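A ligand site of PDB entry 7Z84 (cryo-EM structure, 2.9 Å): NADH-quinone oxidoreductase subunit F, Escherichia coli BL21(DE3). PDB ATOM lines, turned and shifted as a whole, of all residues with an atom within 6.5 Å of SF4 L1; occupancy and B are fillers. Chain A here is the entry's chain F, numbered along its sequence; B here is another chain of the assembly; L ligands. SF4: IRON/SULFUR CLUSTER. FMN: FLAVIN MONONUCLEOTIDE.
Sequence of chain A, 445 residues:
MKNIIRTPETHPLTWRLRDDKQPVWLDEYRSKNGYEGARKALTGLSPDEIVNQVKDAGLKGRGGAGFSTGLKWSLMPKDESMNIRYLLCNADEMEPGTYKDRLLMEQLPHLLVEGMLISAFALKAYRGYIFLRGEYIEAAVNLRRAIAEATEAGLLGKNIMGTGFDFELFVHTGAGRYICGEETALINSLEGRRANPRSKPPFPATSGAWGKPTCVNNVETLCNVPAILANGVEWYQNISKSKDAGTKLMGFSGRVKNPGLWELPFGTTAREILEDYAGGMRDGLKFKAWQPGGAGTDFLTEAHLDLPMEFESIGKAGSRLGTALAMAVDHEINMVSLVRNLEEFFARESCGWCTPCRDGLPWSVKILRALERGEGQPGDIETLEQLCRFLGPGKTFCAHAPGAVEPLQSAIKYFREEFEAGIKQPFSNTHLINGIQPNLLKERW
An iron atom (FE3) of SF4 L1 is bound by the side-chain sulfur of Cys 398 (2.3 Å). An iron atom (FE1) of SF4 L1 is bound by the side-chain sulfur (SG) of Cys 354, 2.3 Å away. A ring nitrogen (ND1) of His 400 lies close to a sulfur (S1) of SF4 L1 (3.6 Å). The side-chain hydroxyl (OG) of Ser 350 sits close to a sulfur (S3) of SF4 L1, at 3.4 Å. SG of Cys 357 is bound to FE2 of SF4 L1 (2.3 Å). The backbone NH of Cys 354 lies close to a sulfur (S3) of SF4 L1, 3.3 Å away. N of Cys 351 sits close to S1 of SF4 L1 (3.5 Å). An iron atom (FE4) of SF4 L1 is bound by the side-chain sulfur of Cys 351. The backbone NH of Trp 353 lies close to a sulfur (S3) of SF4 L1. The backbone NH (N) of Gly 352 sits close to a sulfur (S3) of SF4 L1, 3.7 Å away.
The side-chain hydroxyl (OG) of Ser 350 is in hydrogen-bond range of the backbone NH (N) of Gly 352, at 3.3 Å. NH1 of Arg 358 is in hydrogen-bond range of O of Gly 352 (3.5 Å). The backbone carbonyl oxygen (O) of Trp 353 lies within hydrogen-bond range of the guanidinium group (NH1) of Arg 358 (3.0 Å). SG of Cys 354 sits close to N of Phe 397. N of His 400 lies close to SG of Cys 398, 3.3 Å away. SG of Cys 357 sits close to OG of Ser 350. SG of Cys 351 lies close to ND2 of Asn 196, 3.4 Å away. ND1 of His 400 sits close to SG of Cys 357 (3.2 Å).
Residues that only touch SF4 L1: Pro 197, Phe 397, Ile 179 and Thr 396. Hydrophobic or aromatic side chains within 4 Å of SF4 L1: Ile 179, Pro 197, Phe 397 and His 400. Within 4 Å of SF4 L1: Ile 179, Pro 197, Ser 350, Cys 351, Gly 352, Trp 353, Cys 354, Cys 357, Thr 396, Phe 397, Cys 398 and His 400. The nearest printed residue that does not touch SF4 L1 is Ala 401 (4.1 Å).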
ATOM      1  N   ILE A 179      29.624 -15.703  14.770  1.00  0.00           N
ATOM      2  CA  ILE A 179      28.831 -16.879  15.146  1.00  0.00           C
ATOM      3  C   ILE A 179      27.847 -16.578  16.266  1.00  0.00           C
ATOM      4  O   ILE A 179      26.885 -17.337  16.458  1.00  0.00           O
ATOM      5  CB  ILE A 179      29.785 -18.025  15.512  1.00  0.00           C
ATOM      6  CG1 ILE A 179      29.082 -19.386  15.499  1.00  0.00           C
ATOM      7  CG2 ILE A 179      30.446 -17.781  16.859  1.00  0.00           C
ATOM      8  CD1 ILE A 179      28.142 -19.597  14.335  1.00  0.00           C
ATOM      9  N   ALA A 195      30.739 -18.879  22.255  1.00  0.00           N
ATOM     10  CA  ALA A 195      29.544 -18.893  21.420  1.00  0.00           C
ATOM     11  C   ALA A 195      29.529 -20.113  20.492  1.00  0.00           C
ATOM     12  O   ALA A 195      29.402 -20.014  19.271  1.00  0.00           O
ATOM     13  CB  ALA A 195      29.436 -17.602  20.624  1.00  0.00           C
ATOM     14  N   ASN A 196      29.671 -21.283  21.092  1.00  0.00           N
ATOM     15  CA  ASN A 196      29.385 -22.525  20.389  1.00  0.00           C
ATOM     16  C   ASN A 196      27.888 -22.742  20.337  1.00  0.00           C
ATOM     17  O   ASN A 196      27.212 -22.620  21.360  1.00  0.00           O
ATOM     18  CB  ASN A 196      30.061 -23.711  21.081  1.00  0.00           C
ATOM     19  CG  ASN A 196      31.561 -23.561  21.183  1.00  0.00           C
ATOM     20  OD1 ASN A 196      32.111 -23.391  22.268  1.00  0.00           O
ATOM     21  ND2 ASN A 196      32.239 -23.613  20.045  1.00  0.00           N
ATOM     22  N   PRO A 197      27.321 -23.046  19.173  1.00  0.00           N
ATOM     23  CA  PRO A 197      25.879 -23.317  19.094  1.00  0.00           C
ATOM     24  C   PRO A 197      25.526 -24.639  19.757  1.00  0.00           C
ATOM     25  O   PRO A 197      26.384 -25.417  20.161  1.00  0.00           O
ATOM     26  CB  PRO A 197      25.591 -23.341  17.589  1.00  0.00           C
ATOM     27  CG  PRO A 197      26.899 -23.598  16.948  1.00  0.00           C
ATOM     28  CD  PRO A 197      27.956 -23.038  17.846  1.00  0.00           C
ATOM     29  N   GLU A 349      35.577 -16.874  10.730  1.00  0.00           N
ATOM     30  CA  GLU A 349      34.476 -16.677  11.672  1.00  0.00           C
ATOM     31  C   GLU A 349      33.854 -17.986  12.121  1.00  0.00           C
ATOM     32  O   GLU A 349      32.774 -17.976  12.717  1.00  0.00           O
ATOM     33  CB  GLU A 349      33.408 -15.771  11.053  1.00  0.00           C
ATOM     34  CG  GLU A 349      33.874 -14.340  10.828  1.00  0.00           C
ATOM     35  CD  GLU A 349      34.359 -13.666  12.094  1.00  0.00           C
ATOM     36  OE1 GLU A 349      33.706 -13.823  13.140  1.00  0.00           O
ATOM     37  OE2 GLU A 349      35.404 -12.977  12.042  1.00  0.00           O
ATOM     38  N   SER A 350      34.504 -19.109  11.835  1.00  0.00           N
ATOM     39  CA  SER A 350      34.079 -20.390  12.382  1.00  0.00           C
ATOM     40  C   SER A 350      34.250 -20.394  13.902  1.00  0.00           C
ATOM     41  O   SER A 350      35.136 -19.728  14.445  1.00  0.00           O
ATOM     42  CB  SER A 350      34.878 -21.531  11.755  1.00  0.00           C
ATOM     43  OG  SER A 350      34.507 -22.783  12.314  1.00  0.00           O
ATOM     44  N   CYS A 351      33.389 -21.129  14.580  1.00  0.00           N
ATOM     45  CA  CYS A 351      33.477 -21.221  16.028  1.00  0.00           C
ATOM     46  C   CYS A 351      34.383 -22.352  16.501  1.00  0.00           C
ATOM     47  O   CYS A 351      34.652 -22.444  17.700  1.00  0.00           O
ATOM     48  CB  CYS A 351      32.078 -21.401  16.628  1.00  0.00           C
ATOM     49  SG  CYS A 351      31.536 -23.097  16.737  1.00  0.00           S
ATOM     50  N   GLY A 352      34.845 -23.206  15.586  1.00  0.00           N
ATOM     51  CA  GLY A 352      35.805 -24.236  15.929  1.00  0.00           C
ATOM     52  C   GLY A 352      35.229 -25.479  16.575  1.00  0.00           C
ATOM     53  O   GLY A 352      36.008 -26.331  17.023  1.00  0.00           O
ATOM     54  N   TRP A 353      33.902 -25.611  16.636  1.00  0.00           N
ATOM     55  CA  TRP A 353      33.320 -26.751  17.330  1.00  0.00           C
ATOM     56  C   TRP A 353      33.418 -28.012  16.499  1.00  0.00           C
ATOM     57  O   TRP A 353      33.972 -29.020  16.953  1.00  0.00           O
ATOM     58  CB  TRP A 353      31.863 -26.450  17.677  1.00  0.00           C
ATOM     59  CG  TRP A 353      31.120 -27.601  18.280  1.00  0.00           C
ATOM     60  CD1 TRP A 353      30.125 -28.329  17.692  1.00  0.00           C
ATOM     61  CD2 TRP A 353      31.292 -28.145  19.587  1.00  0.00           C
ATOM     62  NE1 TRP A 353      29.681 -29.298  18.556  1.00  0.00           N
ATOM     63  CE2 TRP A 353      30.385 -29.208  19.723  1.00  0.00           C
ATOM     64  CE3 TRP A 353      32.148 -27.849  20.662  1.00  0.00           C
ATOM     65  CZ2 TRP A 353      30.296 -29.962  20.883  1.00  0.00           C
ATOM     66  CZ3 TRP A 353      32.057 -28.602  21.807  1.00  0.00           C
ATOM     67  CH2 TRP A 353      31.135 -29.656  21.911  1.00  0.00           C
ATOM     68  N   CYS A 354      32.906 -27.987  15.275  1.00  0.00           N
ATOM     69  CA  CYS A 354      32.736 -29.209  14.513  1.00  0.00           C
ATOM     70  C   CYS A 354      33.689 -29.255  13.311  1.00  0.00           C
ATOM     71  O   CYS A 354      34.053 -28.226  12.742  1.00  0.00           O
ATOM     72  CB  CYS A 354      31.277 -29.402  14.072  1.00  0.00           C
ATOM     73  SG  CYS A 354      30.692 -28.480  12.674  1.00  0.00           S
ATOM     74  N   THR A 355      34.086 -30.487  12.967  1.00  0.00           N
ATOM     75  CA  THR A 355      35.200 -30.722  12.056  1.00  0.00           C
ATOM     76  C   THR A 355      35.024 -30.191  10.633  1.00  0.00           C
ATOM     77  O   THR A 355      35.972 -29.561  10.134  1.00  0.00           O
ATOM     78  CB  THR A 355      35.514 -32.228  12.040  1.00  0.00           C
ATOM     79  OG1 THR A 355      35.911 -32.649  13.351  1.00  0.00           O
ATOM     80  CG2 THR A 355      36.630 -32.556  11.060  1.00  0.00           C
ATOM     81  N   PRO A 356      33.909 -30.413   9.902  1.00  0.00           N
ATOM     82  CA  PRO A 356      33.909 -30.053   8.470  1.00  0.00           C
ATOM     83  C   PRO A 356      34.085 -28.572   8.202  1.00  0.00           C
ATOM     84  O   PRO A 356      34.913 -28.217   7.361  1.00  0.00           O
ATOM     85  CB  PRO A 356      32.540 -30.556   7.998  1.00  0.00           C
ATOM     86  CG  PRO A 356      32.166 -31.599   8.939  1.00  0.00           C
ATOM     87  CD  PRO A 356      32.634 -31.070  10.247  1.00  0.00           C
ATOM     88  N   CYS A 357      33.373 -27.701   8.916  1.00  0.00           N
ATOM     89  CA  CYS A 357      33.570 -26.262   8.770  1.00  0.00           C
ATOM     90  C   CYS A 357      34.984 -25.860   9.161  1.00  0.00           C
ATOM     91  O   CYS A 357      35.737 -25.320   8.336  1.00  0.00           O
ATOM     92  CB  CYS A 357      32.516 -25.546   9.610  1.00  0.00           C
ATOM     93  SG  CYS A 357      32.663 -23.800  10.057  1.00  0.00           S
ATOM     94  N   ARG A 358      35.409 -26.258  10.373  1.00  0.00           N
ATOM     95  CA  ARG A 358      36.669 -25.818  10.964  1.00  0.00           C
ATOM     96  C   ARG A 358      37.875 -26.270  10.139  1.00  0.00           C
ATOM     97  O   ARG A 358      38.856 -25.521  10.008  1.00  0.00           O
ATOM     98  CB  ARG A 358      36.761 -26.345  12.395  1.00  0.00           C
ATOM     99  CG  ARG A 358      38.175 -26.573  12.928  1.00  0.00           C
ATOM    100  CD  ARG A 358      38.165 -27.308  14.260  1.00  0.00           C
ATOM    101  NE  ARG A 358      38.340 -28.740  14.081  1.00  0.00           N
ATOM    102  CZ  ARG A 358      37.531 -29.658  14.589  1.00  0.00           C
ATOM    103  NH1 ARG A 358      36.492 -29.331  15.332  1.00  0.00           N
ATOM    104  NH2 ARG A 358      37.782 -30.940  14.348  1.00  0.00           N
ATOM    105  N   LEU A 361      36.796 -25.360   5.542  1.00  0.00           N
ATOM    106  CA  LEU A 361      36.809 -23.983   5.050  1.00  0.00           C
ATOM    107  C   LEU A 361      38.219 -23.428   4.851  1.00  0.00           C
ATOM    108  O   LEU A 361      38.427 -22.756   3.834  1.00  0.00           O
ATOM    109  CB  LEU A 361      35.961 -23.094   5.981  1.00  0.00           C
ATOM    110  CG  LEU A 361      34.462 -23.373   5.950  1.00  0.00           C
ATOM    111  CD1 LEU A 361      33.707 -22.363   6.793  1.00  0.00           C
ATOM    112  CD2 LEU A 361      33.944 -23.379   4.522  1.00  0.00           C
ATOM    113  N   THR A 396      27.323 -30.543   9.132  1.00  0.00           N
ATOM    114  CA  THR A 396      27.961 -29.737  10.161  1.00  0.00           C
ATOM    115  C   THR A 396      26.991 -29.511  11.314  1.00  0.00           C
ATOM    116  O   THR A 396      25.779 -29.717  11.196  1.00  0.00           O
ATOM    117  CB  THR A 396      28.419 -28.398   9.589  1.00  0.00           C
ATOM    118  OG1 THR A 396      27.293 -27.704   9.031  1.00  0.00           O
ATOM    119  CG2 THR A 396      29.446 -28.626   8.509  1.00  0.00           C
ATOM    120  N   PHE A 397      27.551 -29.086  12.450  1.00  0.00           N
ATOM    121  CA  PHE A 397      26.765 -28.965  13.671  1.00  0.00           C
ATOM    122  C   PHE A 397      25.742 -27.837  13.597  1.00  0.00           C
ATOM    123  O   PHE A 397      24.685 -27.930  14.220  1.00  0.00           O
ATOM    124  CB  PHE A 397      27.692 -28.771  14.870  1.00  0.00           C
ATOM    125  CG  PHE A 397      27.003 -28.882  16.190  1.00  0.00           C
ATOM    126  CD1 PHE A 397      26.601 -30.117  16.668  1.00  0.00           C
ATOM    127  CD2 PHE A 397      26.764 -27.763  16.955  1.00  0.00           C
ATOM    128  CE1 PHE A 397      25.979 -30.231  17.887  1.00  0.00           C
ATOM    129  CE2 PHE A 397      26.138 -27.864  18.176  1.00  0.00           C
ATOM    130  CZ  PHE A 397      25.737 -29.104  18.646  1.00  0.00           C
ATOM    131  N   CYS A 398      26.033 -26.786  12.837  1.00  0.00           N
ATOM    132  CA  CYS A 398      25.105 -25.678  12.678  1.00  0.00           C
ATOM    133  C   CYS A 398      25.065 -25.301  11.202  1.00  0.00           C
ATOM    134  O   CYS A 398      25.662 -25.962  10.353  1.00  0.00           O
ATOM    135  CB  CYS A 398      25.502 -24.517  13.595  1.00  0.00           C
ATOM    136  SG  CYS A 398      26.616 -23.303  12.889  1.00  0.00           S
ATOM    137  N   ALA A 399      24.352 -24.218  10.882  1.00  0.00           N
ATOM    138  CA  ALA A 399      24.094 -23.822   9.509  1.00  0.00           C
ATOM    139  C   ALA A 399      25.072 -22.772   8.992  1.00  0.00           C
ATOM    140  O   ALA A 399      24.795 -22.123   7.980  1.00  0.00           O
ATOM    141  CB  ALA A 399      22.665 -23.312   9.355  1.00  0.00           C
ATOM    142  N   HIS A 400      26.204 -22.583   9.674  1.00  0.00           N
ATOM    143  CA  HIS A 400      27.190 -21.614   9.218  1.00  0.00           C
ATOM    144  C   HIS A 400      27.912 -22.090   7.961  1.00  0.00           C
ATOM    145  O   HIS A 400      28.105 -21.315   7.015  1.00  0.00           O
ATOM    146  CB  HIS A 400      28.183 -21.345  10.346  1.00  0.00           C
ATOM    147  CG  HIS A 400      29.452 -20.690   9.902  1.00  0.00           C
ATOM    148  ND1 HIS A 400      30.598 -21.400   9.647  1.00  0.00           N
ATOM    149  CD2 HIS A 400      29.760 -19.390   9.699  1.00  0.00           C
ATOM    150  CE1 HIS A 400      31.557 -20.564   9.286  1.00  0.00           C
ATOM    151  NE2 HIS A 400      31.077 -19.338   9.308  1.00  0.00           N
ATOM    152  N   ALA A 401      28.288 -23.357   7.916  1.00  0.00           N
ATOM    153  CA  ALA A 401      29.012 -23.916   6.772  1.00  0.00           C
ATOM    154  C   ALA A 401      28.168 -24.153   5.517  1.00  0.00           C
ATOM    155  O   ALA A 401      28.716 -24.010   4.416  1.00  0.00           O
ATOM    156  CB  ALA A 401      29.714 -25.217   7.190  1.00  0.00           C
ATOM    157  N   PRO A 402      26.880 -24.551   5.592  1.00  0.00           N
ATOM    158  CA  PRO A 402      26.071 -24.520   4.357  1.00  0.00           C
ATOM    159  C   PRO A 402      25.970 -23.141   3.735  1.00  0.00           C
ATOM    160  O   PRO A 402      26.082 -23.002   2.508  1.00  0.00           O
ATOM    161  CB  PRO A 402      24.698 -25.024   4.838  1.00  0.00           C
ATOM    162  CG  PRO A 402      25.012 -25.921   5.938  1.00  0.00           C
ATOM    163  CD  PRO A 402      26.179 -25.317   6.644  1.00  0.00           C
ATOM    164  N   HIS B 176      38.496 -20.334  15.299  1.00  0.00           N
ATOM    165  CA  HIS B 176      38.053 -21.149  14.169  1.00  0.00           C
ATOM    166  C   HIS B 176      38.808 -22.445  13.902  1.00  0.00           C
ATOM    167  O   HIS B 176      38.210 -23.520  13.918  1.00  0.00           O
ATOM    168  CB  HIS B 176      38.170 -20.263  12.929  1.00  0.00           C
ATOM    169  CG  HIS B 176      39.281 -19.271  13.013  1.00  0.00           C
ATOM    170  ND1 HIS B 176      40.581 -19.578  12.646  1.00  0.00           N
ATOM    171  CD2 HIS B 176      39.306 -17.990  13.447  1.00  0.00           C
ATOM    172  CE1 HIS B 176      41.345 -18.516  12.840  1.00  0.00           C
ATOM    173  NE2 HIS B 176      40.605 -17.537  13.319  1.00  0.00           N
HETATM  174 FE1  SF4 L   1      30.493 -26.203  13.127  1.00  0.00          FE
HETATM  175 FE2  SF4 L   1      31.346 -24.016  11.961  1.00  0.00          FE
HETATM  176 FE3  SF4 L   1      28.820 -24.021  13.051  1.00  0.00          FE
HETATM  177 FE4  SF4 L   1      30.931 -23.946  14.654  1.00  0.00          FE
HETATM  178  S1  SF4 L   1      30.362 -22.297  13.147  1.00  0.00           S
HETATM  179  S2  SF4 L   1      29.179 -25.424  14.846  1.00  0.00           S
HETATM  180  S3  SF4 L   1      32.514 -25.199  13.552  1.00  0.00           S
HETATM  181  S4  SF4 L   1      29.535 -25.261  11.270  1.00  0.00           S
HETATM  182  N1  FMN L   2      19.889 -13.907  12.977  1.00  0.00           N
HETATM  183  C2  FMN L   2      19.927 -12.565  13.280  1.00  0.00           C
HETATM  184  O2  FMN L   2      18.885 -11.969  13.496  1.00  0.00           O
HETATM  185  N3  FMN L   2      21.136 -11.905  13.337  1.00  0.00           N
HETATM  186  C4  FMN L   2      22.309 -12.600  13.088  1.00  0.00           C
HETATM  187  O4  FMN L   2      23.381 -12.008  13.137  1.00  0.00           O
HETATM  188  C4A FMN L   2      22.261 -13.945  12.785  1.00  0.00           C
HETATM  189  N5  FMN L   2      23.423 -14.635  12.531  1.00  0.00           N
HETATM  190  C5A FMN L   2      23.377 -15.987  12.235  1.00  0.00           C
HETATM  191  C6  FMN L   2      24.552 -16.652  11.989  1.00  0.00           C
HETATM  192  C7  FMN L   2      24.537 -18.001  11.683  1.00  0.00           C
HETATM  193  C7M FMN L   2      25.822 -18.721  11.419  1.00  0.00           C
HETATM  194  C8  FMN L   2      23.323 -18.678  11.625  1.00  0.00           C
HETATM  195  C8M FMN L   2      23.286 -20.140  11.286  1.00  0.00           C
HETATM  196  C9  FMN L   2      22.134 -18.002  11.873  1.00  0.00           C
HETATM  197  C9A FMN L   2      22.159 -16.650  12.179  1.00  0.00           C
HETATM  198  N10 FMN L   2      20.985 -15.955  12.428  1.00  0.00           N
HETATM  199  C10 FMN L   2      21.043 -14.608  12.729  1.00  0.00           C
HETATM  200  C1' FMN L   2      19.645 -16.625  12.384  1.00  0.00           C
HETATM  201  C2' FMN L   2      19.248 -17.102  13.780  1.00  0.00           C
HETATM  202  O2' FMN L   2      19.661 -18.438  13.967  1.00  0.00           O
HETATM  203  C3' FMN L   2      17.739 -17.000  14.017  1.00  0.00           C
HETATM  204  O3' FMN L   2      17.067 -17.409  12.852  1.00  0.00           O
HETATM  205  C4' FMN L   2      17.357 -15.572  14.368  1.00  0.00           C
HETATM  206  O4' FMN L   2      18.264 -15.055  15.313  1.00  0.00           O
HETATM  207  C5' FMN L   2      15.944 -15.437  14.920  1.00  0.00           C
HETATM  208  O5' FMN L   2      15.005 -15.975  14.011  1.00  0.00           O
HETATM  209  P   FMN L   2      13.865 -15.039  13.397  1.00  0.00           P
HETATM  210  O1P FMN L   2      14.192 -14.798  11.952  1.00  0.00           O
HETATM  211  O2P FMN L   2      12.513 -15.700  13.520  1.00  0.00           O
HETATM  212  O3P FMN L   2      13.833 -13.712  14.114  1.00  0.00           O
